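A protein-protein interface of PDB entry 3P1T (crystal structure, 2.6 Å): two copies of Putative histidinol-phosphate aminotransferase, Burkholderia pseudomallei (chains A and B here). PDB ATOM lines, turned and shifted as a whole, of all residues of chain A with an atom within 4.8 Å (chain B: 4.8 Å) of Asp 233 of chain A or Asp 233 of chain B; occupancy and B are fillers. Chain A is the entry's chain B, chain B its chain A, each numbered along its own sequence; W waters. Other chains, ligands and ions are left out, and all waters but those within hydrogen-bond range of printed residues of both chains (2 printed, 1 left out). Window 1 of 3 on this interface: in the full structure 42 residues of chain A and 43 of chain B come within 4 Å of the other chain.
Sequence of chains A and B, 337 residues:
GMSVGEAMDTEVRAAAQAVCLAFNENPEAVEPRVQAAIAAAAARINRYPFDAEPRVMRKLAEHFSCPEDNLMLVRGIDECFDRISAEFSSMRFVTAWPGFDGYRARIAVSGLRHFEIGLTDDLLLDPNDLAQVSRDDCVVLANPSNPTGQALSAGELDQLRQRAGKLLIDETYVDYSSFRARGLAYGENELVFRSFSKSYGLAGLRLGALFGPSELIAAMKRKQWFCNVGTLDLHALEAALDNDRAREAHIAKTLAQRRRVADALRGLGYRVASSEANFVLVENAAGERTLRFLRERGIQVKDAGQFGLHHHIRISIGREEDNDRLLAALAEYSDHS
Printed residues of chain B within 4 Å of Asp 233 of chain A: Asp 233 (3.5 Å). Of the printed residues of chain A, Asp 233 of chain B touches Asp 233 (3.5 Å). Of the printed residues of chain A, Leu 205 of chain B touches Thr 231 (3.9 Å) and Leu 232 (3.7 Å). Of the printed residues of chain B, Arg 75 of chain A touches Arg 75. Printed residues of chain B within 4 Å of Thr 231 of chain A: Leu 205. Printed residues of chain A within 4 Å of Thr 231 of chain B: Leu 205. Printed residues of chain B within 4 Å of Leu 205 of chain A: Thr 231 (3.9 Å) and Leu 232 (3.8 Å). Leu 207 of chain B touches none of the printed residues of chain A. Val 229 of chain A touches none of the printed residues of chain B. The nearest printed residue of chain B that does not touch Asp 233 of chain A is Leu 232 of chain B (4.02 Å). The nearest residue of chain A that does not touch Asp 233 of chain B is Leu 232 of chain A (4.02 Å). The nearest printed residue of chain B that does not touch Thr 231 of chain A is Asp 233 of chain B (5.9 Å).
Arg 75 of chain B touches its own counterpart, Arg 75 of chain A. Leu 205 of chain A touches Thr 231 of chain B, and with the chains exchanged Thr 231 of chain A touches Leu 205 of chain B. Leu 232 of chain A touches its own counterpart, Leu 232 of chain B. Asp 233 of chain A touches its own counterpart, Asp 233 of chain B. Of the 7 pairs that touch across the chains among the printed residues, 7 have their exchanged pair printed and touching as well.
Water W2 lies within hydrogen-bond range of the side-chain carboxylate of Asp 233 of chain B (2.5 Å), the backbone NH of Asp 233 of chain A (3.1 Å) and the backbone NH of Leu 232 of chain A (3.3 Å). Water W1 lies within hydrogen-bond range of OD1 of Asp 233 of chain A (2.6 Å), N of Leu 232 of chain B (3.0 Å), N of Asp 233 of chain B (3.0 Å) and O of Gly 230 of chain B (3.5 Å).
Of the 12 printed residues of chain B, 5 touch a printed residue of chain A. Hydrophobic or aromatic side chains of chain B within 4 Å of the printed part of chain A: Leu 205 and Leu 232. Hydrophobic or aromatic side chains of chain A that line the printed part of chain B: Leu 205 and Leu 232. Among the printed residues, no Asp or Glu carboxylate lies within 4 Å of a Lys or Arg side-chain nitrogen of the other chain.
The backbone carbonyl oxygen of Leu 205 of chain B sits at hydrogen-bond distance from the guanidinium group of Arg 75 of chain B (2.8 Å). The backbone carbonyl oxygen (O) of Thr 231 of chain A sits at hydrogen-bond distance from a ring nitrogen (ND1) of His 235 of chain A (2.7 Å). The side-chain carboxylate (OD2) of Asp 233 of chain A is in salt-bridge range of the guanidinium group (NH2) of Arg 75 of chain A. The backbone carbonyl oxygen of Thr 231 of chain B lies within hydrogen-bond range of a ring nitrogen (ND1) of His 235 of chain B, at 2.7 Å. The guanidinium group (NH2) of Arg 75 of chain B is in salt-bridge range of the side-chain carboxylate (OD2) of Asp 233 of chain B, 2.5 Å away. NH2 of Arg 75 of chain A lies within hydrogen-bond range of O of Leu 205 of chain A, at 2.8 Å.
Among the printed residues, pairs that only touch across the chains: Asp 233 of chain A with Asp 233 of chain B (3.5 Å), Leu 232 of chain A with Leu 205 of chain B (3.7 Å), Leu 205 of chain A with Leu 232 of chain B (3.8 Å), Leu 232 of chain A with Leu 232 of chain B (3.9 Å), Thr 231 of chain A with Leu 205 of chain B (3.9 Å) and Leu 205 of chain A with Thr 231 of chain B (3.9 Å).
The guanidinium group of Arg 75 of chain A lies close to the guanidinium group of Arg 75 of chain B.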
ATOM      1  N   ARG A  75     -15.093 -17.061 -24.221  1.00  0.00           N
ATOM      2  CA  ARG A  75     -15.256 -16.425 -22.920  1.00  0.00           C
ATOM      3  C   ARG A  75     -16.602 -15.662 -22.901  1.00  0.00           C
ATOM      4  O   ARG A  75     -16.635 -14.415 -22.899  1.00  0.00           O
ATOM      5  CB  ARG A  75     -14.071 -15.484 -22.641  1.00  0.00           C
ATOM      6  CG  ARG A  75     -13.865 -15.168 -21.166  1.00  0.00           C
ATOM      7  CD  ARG A  75     -12.756 -16.047 -20.643  1.00  0.00           C
ATOM      8  NE  ARG A  75     -13.211 -17.043 -19.686  1.00  0.00           N
ATOM      9  CZ  ARG A  75     -12.454 -18.021 -19.210  1.00  0.00           C
ATOM     10  NH1 ARG A  75     -11.210 -18.172 -19.639  1.00  0.00           N
ATOM     11  NH2 ARG A  75     -12.941 -18.870 -18.322  1.00  0.00           N
ATOM     12  N   LEU A 205     -17.331 -19.099 -14.345  1.00  0.00           N
ATOM     13  CA  LEU A 205     -16.250 -19.388 -15.298  1.00  0.00           C
ATOM     14  C   LEU A 205     -16.450 -18.611 -16.591  1.00  0.00           C
ATOM     15  O   LEU A 205     -15.486 -18.396 -17.320  1.00  0.00           O
ATOM     16  CB  LEU A 205     -16.122 -20.885 -15.602  1.00  0.00           C
ATOM     17  CG  LEU A 205     -16.058 -21.836 -14.396  1.00  0.00           C
ATOM     18  CD1 LEU A 205     -15.705 -23.219 -14.844  1.00  0.00           C
ATOM     19  CD2 LEU A 205     -15.065 -21.359 -13.340  1.00  0.00           C
ATOM     20  N   LEU A 207     -18.125 -19.206 -19.636  1.00  0.00           N
ATOM     21  CA  LEU A 207     -17.794 -19.989 -20.838  1.00  0.00           C
ATOM     22  C   LEU A 207     -19.038 -20.146 -21.707  1.00  0.00           C
ATOM     23  O   LEU A 207     -20.170 -20.129 -21.208  1.00  0.00           O
ATOM     24  CB  LEU A 207     -17.197 -21.379 -20.494  1.00  0.00           C
ATOM     25  CG  LEU A 207     -15.892 -21.412 -19.711  1.00  0.00           C
ATOM     26  CD1 LEU A 207     -15.527 -22.823 -19.313  1.00  0.00           C
ATOM     27  CD2 LEU A 207     -14.772 -20.752 -20.491  1.00  0.00           C
ATOM     28  N   VAL A 229      -8.677 -20.438 -22.522  1.00  0.00           N
ATOM     29  CA  VAL A 229      -9.364 -21.115 -21.427  1.00  0.00           C
ATOM     30  C   VAL A 229      -8.325 -22.011 -20.715  1.00  0.00           C
ATOM     31  O   VAL A 229      -7.826 -22.972 -21.303  1.00  0.00           O
ATOM     32  CB  VAL A 229     -10.619 -21.899 -21.929  1.00  0.00           C
ATOM     33  CG1 VAL A 229     -11.323 -22.610 -20.775  1.00  0.00           C
ATOM     34  CG2 VAL A 229     -11.599 -20.981 -22.671  1.00  0.00           C
ATOM     35  N   GLY A 230      -8.000 -21.662 -19.472  1.00  0.00           N
ATOM     36  CA  GLY A 230      -7.017 -22.384 -18.665  1.00  0.00           C
ATOM     37  C   GLY A 230      -7.376 -23.808 -18.258  1.00  0.00           C
ATOM     38  O   GLY A 230      -8.521 -24.240 -18.401  1.00  0.00           O
ATOM     39  N   THR A 231      -6.393 -24.530 -17.717  1.00  0.00           N
ATOM     40  CA  THR A 231      -6.504 -25.923 -17.276  1.00  0.00           C
ATOM     41  C   THR A 231      -7.654 -26.116 -16.230  1.00  0.00           C
ATOM     42  O   THR A 231      -8.356 -27.110 -16.328  1.00  0.00           O
ATOM     43  CB  THR A 231      -5.163 -26.434 -16.722  1.00  0.00           C
ATOM     44  OG1 THR A 231      -5.363 -27.730 -16.175  1.00  0.00           O
ATOM     45  CG2 THR A 231      -4.546 -25.529 -15.658  1.00  0.00           C
ATOM     46  N   LEU A 232      -7.870 -25.183 -15.279  1.00  0.00           N
ATOM     47  CA  LEU A 232      -8.932 -25.327 -14.283  1.00  0.00           C
ATOM     48  C   LEU A 232     -10.325 -25.224 -14.930  1.00  0.00           C
ATOM     49  O   LEU A 232     -11.153 -26.099 -14.686  1.00  0.00           O
ATOM     50  CB  LEU A 232      -8.793 -24.295 -13.151  1.00  0.00           C
ATOM     51  CG  LEU A 232      -7.526 -24.377 -12.284  1.00  0.00           C
ATOM     52  CD1 LEU A 232      -7.468 -23.202 -11.322  1.00  0.00           C
ATOM     53  CD2 LEU A 232      -7.406 -25.732 -11.558  1.00  0.00           C
ATOM     54  N   ASP A 233     -10.574 -24.204 -15.775  1.00  0.00           N
ATOM     55  CA  ASP A 233     -11.872 -24.047 -16.455  1.00  0.00           C
ATOM     56  C   ASP A 233     -12.149 -25.215 -17.428  1.00  0.00           C
ATOM     57  O   ASP A 233     -13.291 -25.693 -17.504  1.00  0.00           O
ATOM     58  CB  ASP A 233     -11.948 -22.705 -17.214  1.00  0.00           C
ATOM     59  CG  ASP A 233     -11.876 -21.464 -16.337  1.00  0.00           C
ATOM     60  OD1 ASP A 233     -12.196 -21.571 -15.124  1.00  0.00           O
ATOM     61  OD2 ASP A 233     -11.504 -20.383 -16.863  1.00  0.00           O
ATOM     62  N   LEU A 234     -11.107 -25.681 -18.144  1.00  0.00           N
ATOM     63  CA  LEU A 234     -11.236 -26.792 -19.085  1.00  0.00           C
ATOM     64  C   LEU A 234     -11.661 -28.085 -18.356  1.00  0.00           C
ATOM     65  O   LEU A 234     -12.578 -28.759 -18.824  1.00  0.00           O
ATOM     66  CB  LEU A 234      -9.921 -27.032 -19.869  1.00  0.00           C
ATOM     67  CG  LEU A 234      -9.512 -26.042 -20.947  1.00  0.00           C
ATOM     68  CD1 LEU A 234      -8.081 -26.306 -21.407  1.00  0.00           C
ATOM     69  CD2 LEU A 234     -10.431 -26.130 -22.130  1.00  0.00           C
ATOM     70  N   HIS A 235     -11.015 -28.428 -17.226  1.00  0.00           N
ATOM     71  CA  HIS A 235     -11.353 -29.654 -16.500  1.00  0.00           C
ATOM     72  C   HIS A 235     -12.731 -29.542 -15.829  1.00  0.00           C
ATOM     73  O   HIS A 235     -13.418 -30.563 -15.715  1.00  0.00           O
ATOM     74  CB  HIS A 235     -10.278 -30.029 -15.474  1.00  0.00           C
ATOM     75  CG  HIS A 235      -9.054 -30.599 -16.139  1.00  0.00           C
ATOM     76  ND1 HIS A 235      -8.080 -29.779 -16.672  1.00  0.00           N
ATOM     77  CD2 HIS A 235      -8.734 -31.884 -16.414  1.00  0.00           C
ATOM     78  CE1 HIS A 235      -7.177 -30.588 -17.199  1.00  0.00           C
ATOM     79  NE2 HIS A 235      -7.538 -31.861 -17.085  1.00  0.00           N
ATOM     80  N   ALA A 236     -13.159 -28.325 -15.426  1.00  0.00           N
ATOM     81  CA  ALA A 236     -14.493 -28.111 -14.848  1.00  0.00           C
ATOM     82  C   ALA A 236     -15.554 -28.343 -15.923  1.00  0.00           C
ATOM     83  O   ALA A 236     -16.475 -29.140 -15.700  1.00  0.00           O
ATOM     84  CB  ALA A 236     -14.619 -26.703 -14.262  1.00  0.00           C
ATOM     85  N   LEU A 237     -15.392 -27.677 -17.108  1.00  0.00           N
ATOM     86  CA  LEU A 237     -16.300 -27.814 -18.246  1.00  0.00           C
ATOM     87  C   LEU A 237     -16.413 -29.285 -18.674  1.00  0.00           C
ATOM     88  O   LEU A 237     -17.529 -29.773 -18.855  1.00  0.00           O
ATOM     89  CB  LEU A 237     -15.847 -26.938 -19.438  1.00  0.00           C
ATOM     90  CG  LEU A 237     -16.674 -27.055 -20.716  1.00  0.00           C
ATOM     91  CD1 LEU A 237     -18.090 -26.612 -20.491  1.00  0.00           C
ATOM     92  CD2 LEU A 237     -16.015 -26.306 -21.853  1.00  0.00           C
ATOM     93  N   ARG B  75      -5.459 -11.928 -19.763  1.00  0.00           N
ATOM     94  CA  ARG B  75      -5.275 -13.303 -20.205  1.00  0.00           C
ATOM     95  C   ARG B  75      -3.938 -13.415 -20.980  1.00  0.00           C
ATOM     96  O   ARG B  75      -3.937 -13.609 -22.217  1.00  0.00           O
ATOM     97  CB  ARG B  75      -6.460 -13.743 -21.069  1.00  0.00           C
ATOM     98  CG  ARG B  75      -6.627 -15.250 -21.168  1.00  0.00           C
ATOM     99  CD  ARG B  75      -7.724 -15.650 -20.220  1.00  0.00           C
ATOM    100  NE  ARG B  75      -7.229 -16.446 -19.113  1.00  0.00           N
ATOM    101  CZ  ARG B  75      -7.953 -16.784 -18.059  1.00  0.00           C
ATOM    102  NH1 ARG B  75      -9.205 -16.355 -17.935  1.00  0.00           N
ATOM    103  NH2 ARG B  75      -7.423 -17.522 -17.103  1.00  0.00           N
ATOM    104  N   LEU B 205      -2.890 -21.335 -16.379  1.00  0.00           N
ATOM    105  CA  LEU B 205      -4.010 -20.383 -16.233  1.00  0.00           C
ATOM    106  C   LEU B 205      -3.857 -19.221 -17.193  1.00  0.00           C
ATOM    107  O   LEU B 205      -4.847 -18.546 -17.500  1.00  0.00           O
ATOM    108  CB  LEU B 205      -4.147 -19.857 -14.801  1.00  0.00           C
ATOM    109  CG  LEU B 205      -4.185 -20.905 -13.689  1.00  0.00           C
ATOM    110  CD1 LEU B 205      -4.523 -20.263 -12.388  1.00  0.00           C
ATOM    111  CD2 LEU B 205      -5.166 -22.032 -14.001  1.00  0.00           C
ATOM    112  N   LEU B 207      -2.252 -16.051 -17.040  1.00  0.00           N
ATOM    113  CA  LEU B 207      -2.597 -14.768 -16.437  1.00  0.00           C
ATOM    114  C   LEU B 207      -1.377 -13.850 -16.406  1.00  0.00           C
ATOM    115  O   LEU B 207      -0.227 -14.316 -16.339  1.00  0.00           O
ATOM    116  CB  LEU B 207      -3.168 -14.926 -15.013  1.00  0.00           C
ATOM    117  CG  LEU B 207      -4.449 -15.717 -14.848  1.00  0.00           C
ATOM    118  CD1 LEU B 207      -4.782 -15.899 -13.394  1.00  0.00           C
ATOM    119  CD2 LEU B 207      -5.604 -15.063 -15.574  1.00  0.00           C
ATOM    120  N   VAL B 229     -11.723 -13.133 -16.092  1.00  0.00           N
ATOM    121  CA  VAL B 229     -11.000 -14.101 -15.248  1.00  0.00           C
ATOM    122  C   VAL B 229     -11.997 -14.670 -14.220  1.00  0.00           C
ATOM    123  O   VAL B 229     -12.506 -13.953 -13.367  1.00  0.00           O
ATOM    124  CB  VAL B 229      -9.746 -13.483 -14.586  1.00  0.00           C
ATOM    125  CG1 VAL B 229      -9.004 -14.512 -13.739  1.00  0.00           C
ATOM    126  CG2 VAL B 229      -8.817 -12.901 -15.642  1.00  0.00           C
ATOM    127  N   GLY B 230     -12.304 -15.942 -14.368  1.00  0.00           N
ATOM    128  CA  GLY B 230     -13.266 -16.648 -13.529  1.00  0.00           C
ATOM    129  C   GLY B 230     -12.854 -16.876 -12.093  1.00  0.00           C
ATOM    130  O   GLY B 230     -11.707 -16.651 -11.713  1.00  0.00           O
ATOM    131  N   THR B 231     -13.801 -17.359 -11.298  1.00  0.00           N
ATOM    132  CA  THR B 231     -13.648 -17.619  -9.868  1.00  0.00           C
ATOM    133  C   THR B 231     -12.486 -18.607  -9.555  1.00  0.00           C
ATOM    134  O   THR B 231     -11.786 -18.373  -8.573  1.00  0.00           O
ATOM    135  CB  THR B 231     -14.958 -18.136  -9.271  1.00  0.00           C
ATOM    136  OG1 THR B 231     -14.717 -18.532  -7.918  1.00  0.00           O
ATOM    137  CG2 THR B 231     -15.556 -19.286 -10.047  1.00  0.00           C
ATOM    138  N   LEU B 232     -12.261 -19.657 -10.372  1.00  0.00           N
ATOM    139  CA  LEU B 232     -11.173 -20.615 -10.108  1.00  0.00           C
ATOM    140  C   LEU B 232      -9.793 -19.947 -10.306  1.00  0.00           C
ATOM    141  O   LEU B 232      -8.931 -20.064  -9.430  1.00  0.00           O
ATOM    142  CB  LEU B 232     -11.278 -21.880 -10.990  1.00  0.00           C
ATOM    143  CG  LEU B 232     -12.504 -22.762 -10.797  1.00  0.00           C
ATOM    144  CD1 LEU B 232     -12.550 -23.856 -11.841  1.00  0.00           C
ATOM    145  CD2 LEU B 232     -12.558 -23.332  -9.378  1.00  0.00           C
ATOM    146  N   ASP B 233      -9.603 -19.216 -11.426  1.00  0.00           N
ATOM    147  CA  ASP B 233      -8.339 -18.552 -11.715  1.00  0.00           C
ATOM    148  C   ASP B 233      -8.073 -17.425 -10.709  1.00  0.00           C
ATOM    149  O   ASP B 233      -6.930 -17.275 -10.268  1.00  0.00           O
ATOM    150  CB  ASP B 233      -8.323 -18.022 -13.152  1.00  0.00           C
ATOM    151  CG  ASP B 233      -8.397 -19.075 -14.248  1.00  0.00           C
ATOM    152  OD1 ASP B 233      -8.056 -20.238 -13.979  1.00  0.00           O
ATOM    153  OD2 ASP B 233      -8.796 -18.729 -15.373  1.00  0.00           O
ATOM    154  N   LEU B 234      -9.119 -16.679 -10.310  1.00  0.00           N
ATOM    155  CA  LEU B 234      -8.999 -15.602  -9.316  1.00  0.00           C
ATOM    156  C   LEU B 234      -8.548 -16.129  -7.938  1.00  0.00           C
ATOM    157  O   LEU B 234      -7.625 -15.553  -7.360  1.00  0.00           O
ATOM    158  CB  LEU B 234     -10.312 -14.830  -9.147  1.00  0.00           C
ATOM    159  CG  LEU B 234     -10.746 -13.884 -10.276  1.00  0.00           C
ATOM    160  CD1 LEU B 234     -12.146 -13.421 -10.040  1.00  0.00           C
ATOM    161  CD2 LEU B 234      -9.837 -12.697 -10.393  1.00  0.00           C
ATOM    162  N   HIS B 235      -9.151 -17.226  -7.428  1.00  0.00           N
ATOM    163  CA  HIS B 235      -8.734 -17.795  -6.133  1.00  0.00           C
ATOM    164  C   HIS B 235      -7.347 -18.423  -6.227  1.00  0.00           C
ATOM    165  O   HIS B 235      -6.615 -18.406  -5.241  1.00  0.00           O
ATOM    166  CB  HIS B 235      -9.740 -18.812  -5.597  1.00  0.00           C
ATOM    167  CG  HIS B 235     -10.976 -18.137  -5.085  1.00  0.00           C
ATOM    168  ND1 HIS B 235     -11.995 -17.749  -5.938  1.00  0.00           N
ATOM    169  CD2 HIS B 235     -11.273 -17.707  -3.838  1.00  0.00           C
ATOM    170  CE1 HIS B 235     -12.888 -17.139  -5.182  1.00  0.00           C
ATOM    171  NE2 HIS B 235     -12.496 -17.084  -3.914  1.00  0.00           N
ATOM    172  N   ALA B 236      -6.973 -18.917  -7.413  1.00  0.00           N
ATOM    173  CA  ALA B 236      -5.655 -19.487  -7.654  1.00  0.00           C
ATOM    174  C   ALA B 236      -4.592 -18.381  -7.564  1.00  0.00           C
ATOM    175  O   ALA B 236      -3.673 -18.471  -6.729  1.00  0.00           O
ATOM    176  CB  ALA B 236      -5.618 -20.175  -9.007  1.00  0.00           C
ATOM    177  N   LEU B 237      -4.788 -17.295  -8.352  1.00  0.00           N
ATOM    178  CA  LEU B 237      -3.904 -16.139  -8.394  1.00  0.00           C
ATOM    179  C   LEU B 237      -3.743 -15.527  -7.002  1.00  0.00           C
ATOM    180  O   LEU B 237      -2.602 -15.267  -6.581  1.00  0.00           O
ATOM    181  CB  LEU B 237      -4.423 -15.089  -9.384  1.00  0.00           C
ATOM    182  CG  LEU B 237      -3.625 -13.789  -9.465  1.00  0.00           C
ATOM    183  CD1 LEU B 237      -2.217 -14.039  -9.904  1.00  0.00           C
ATOM    184  CD2 LEU B 237      -4.282 -12.812 -10.378  1.00  0.00           C
HETATM  185  O   HOH W   1     -11.864 -19.731 -13.312  1.00  0.00           O
HETATM  186  O   HOH W   2      -8.478 -21.941 -15.753  1.00  0.00           O
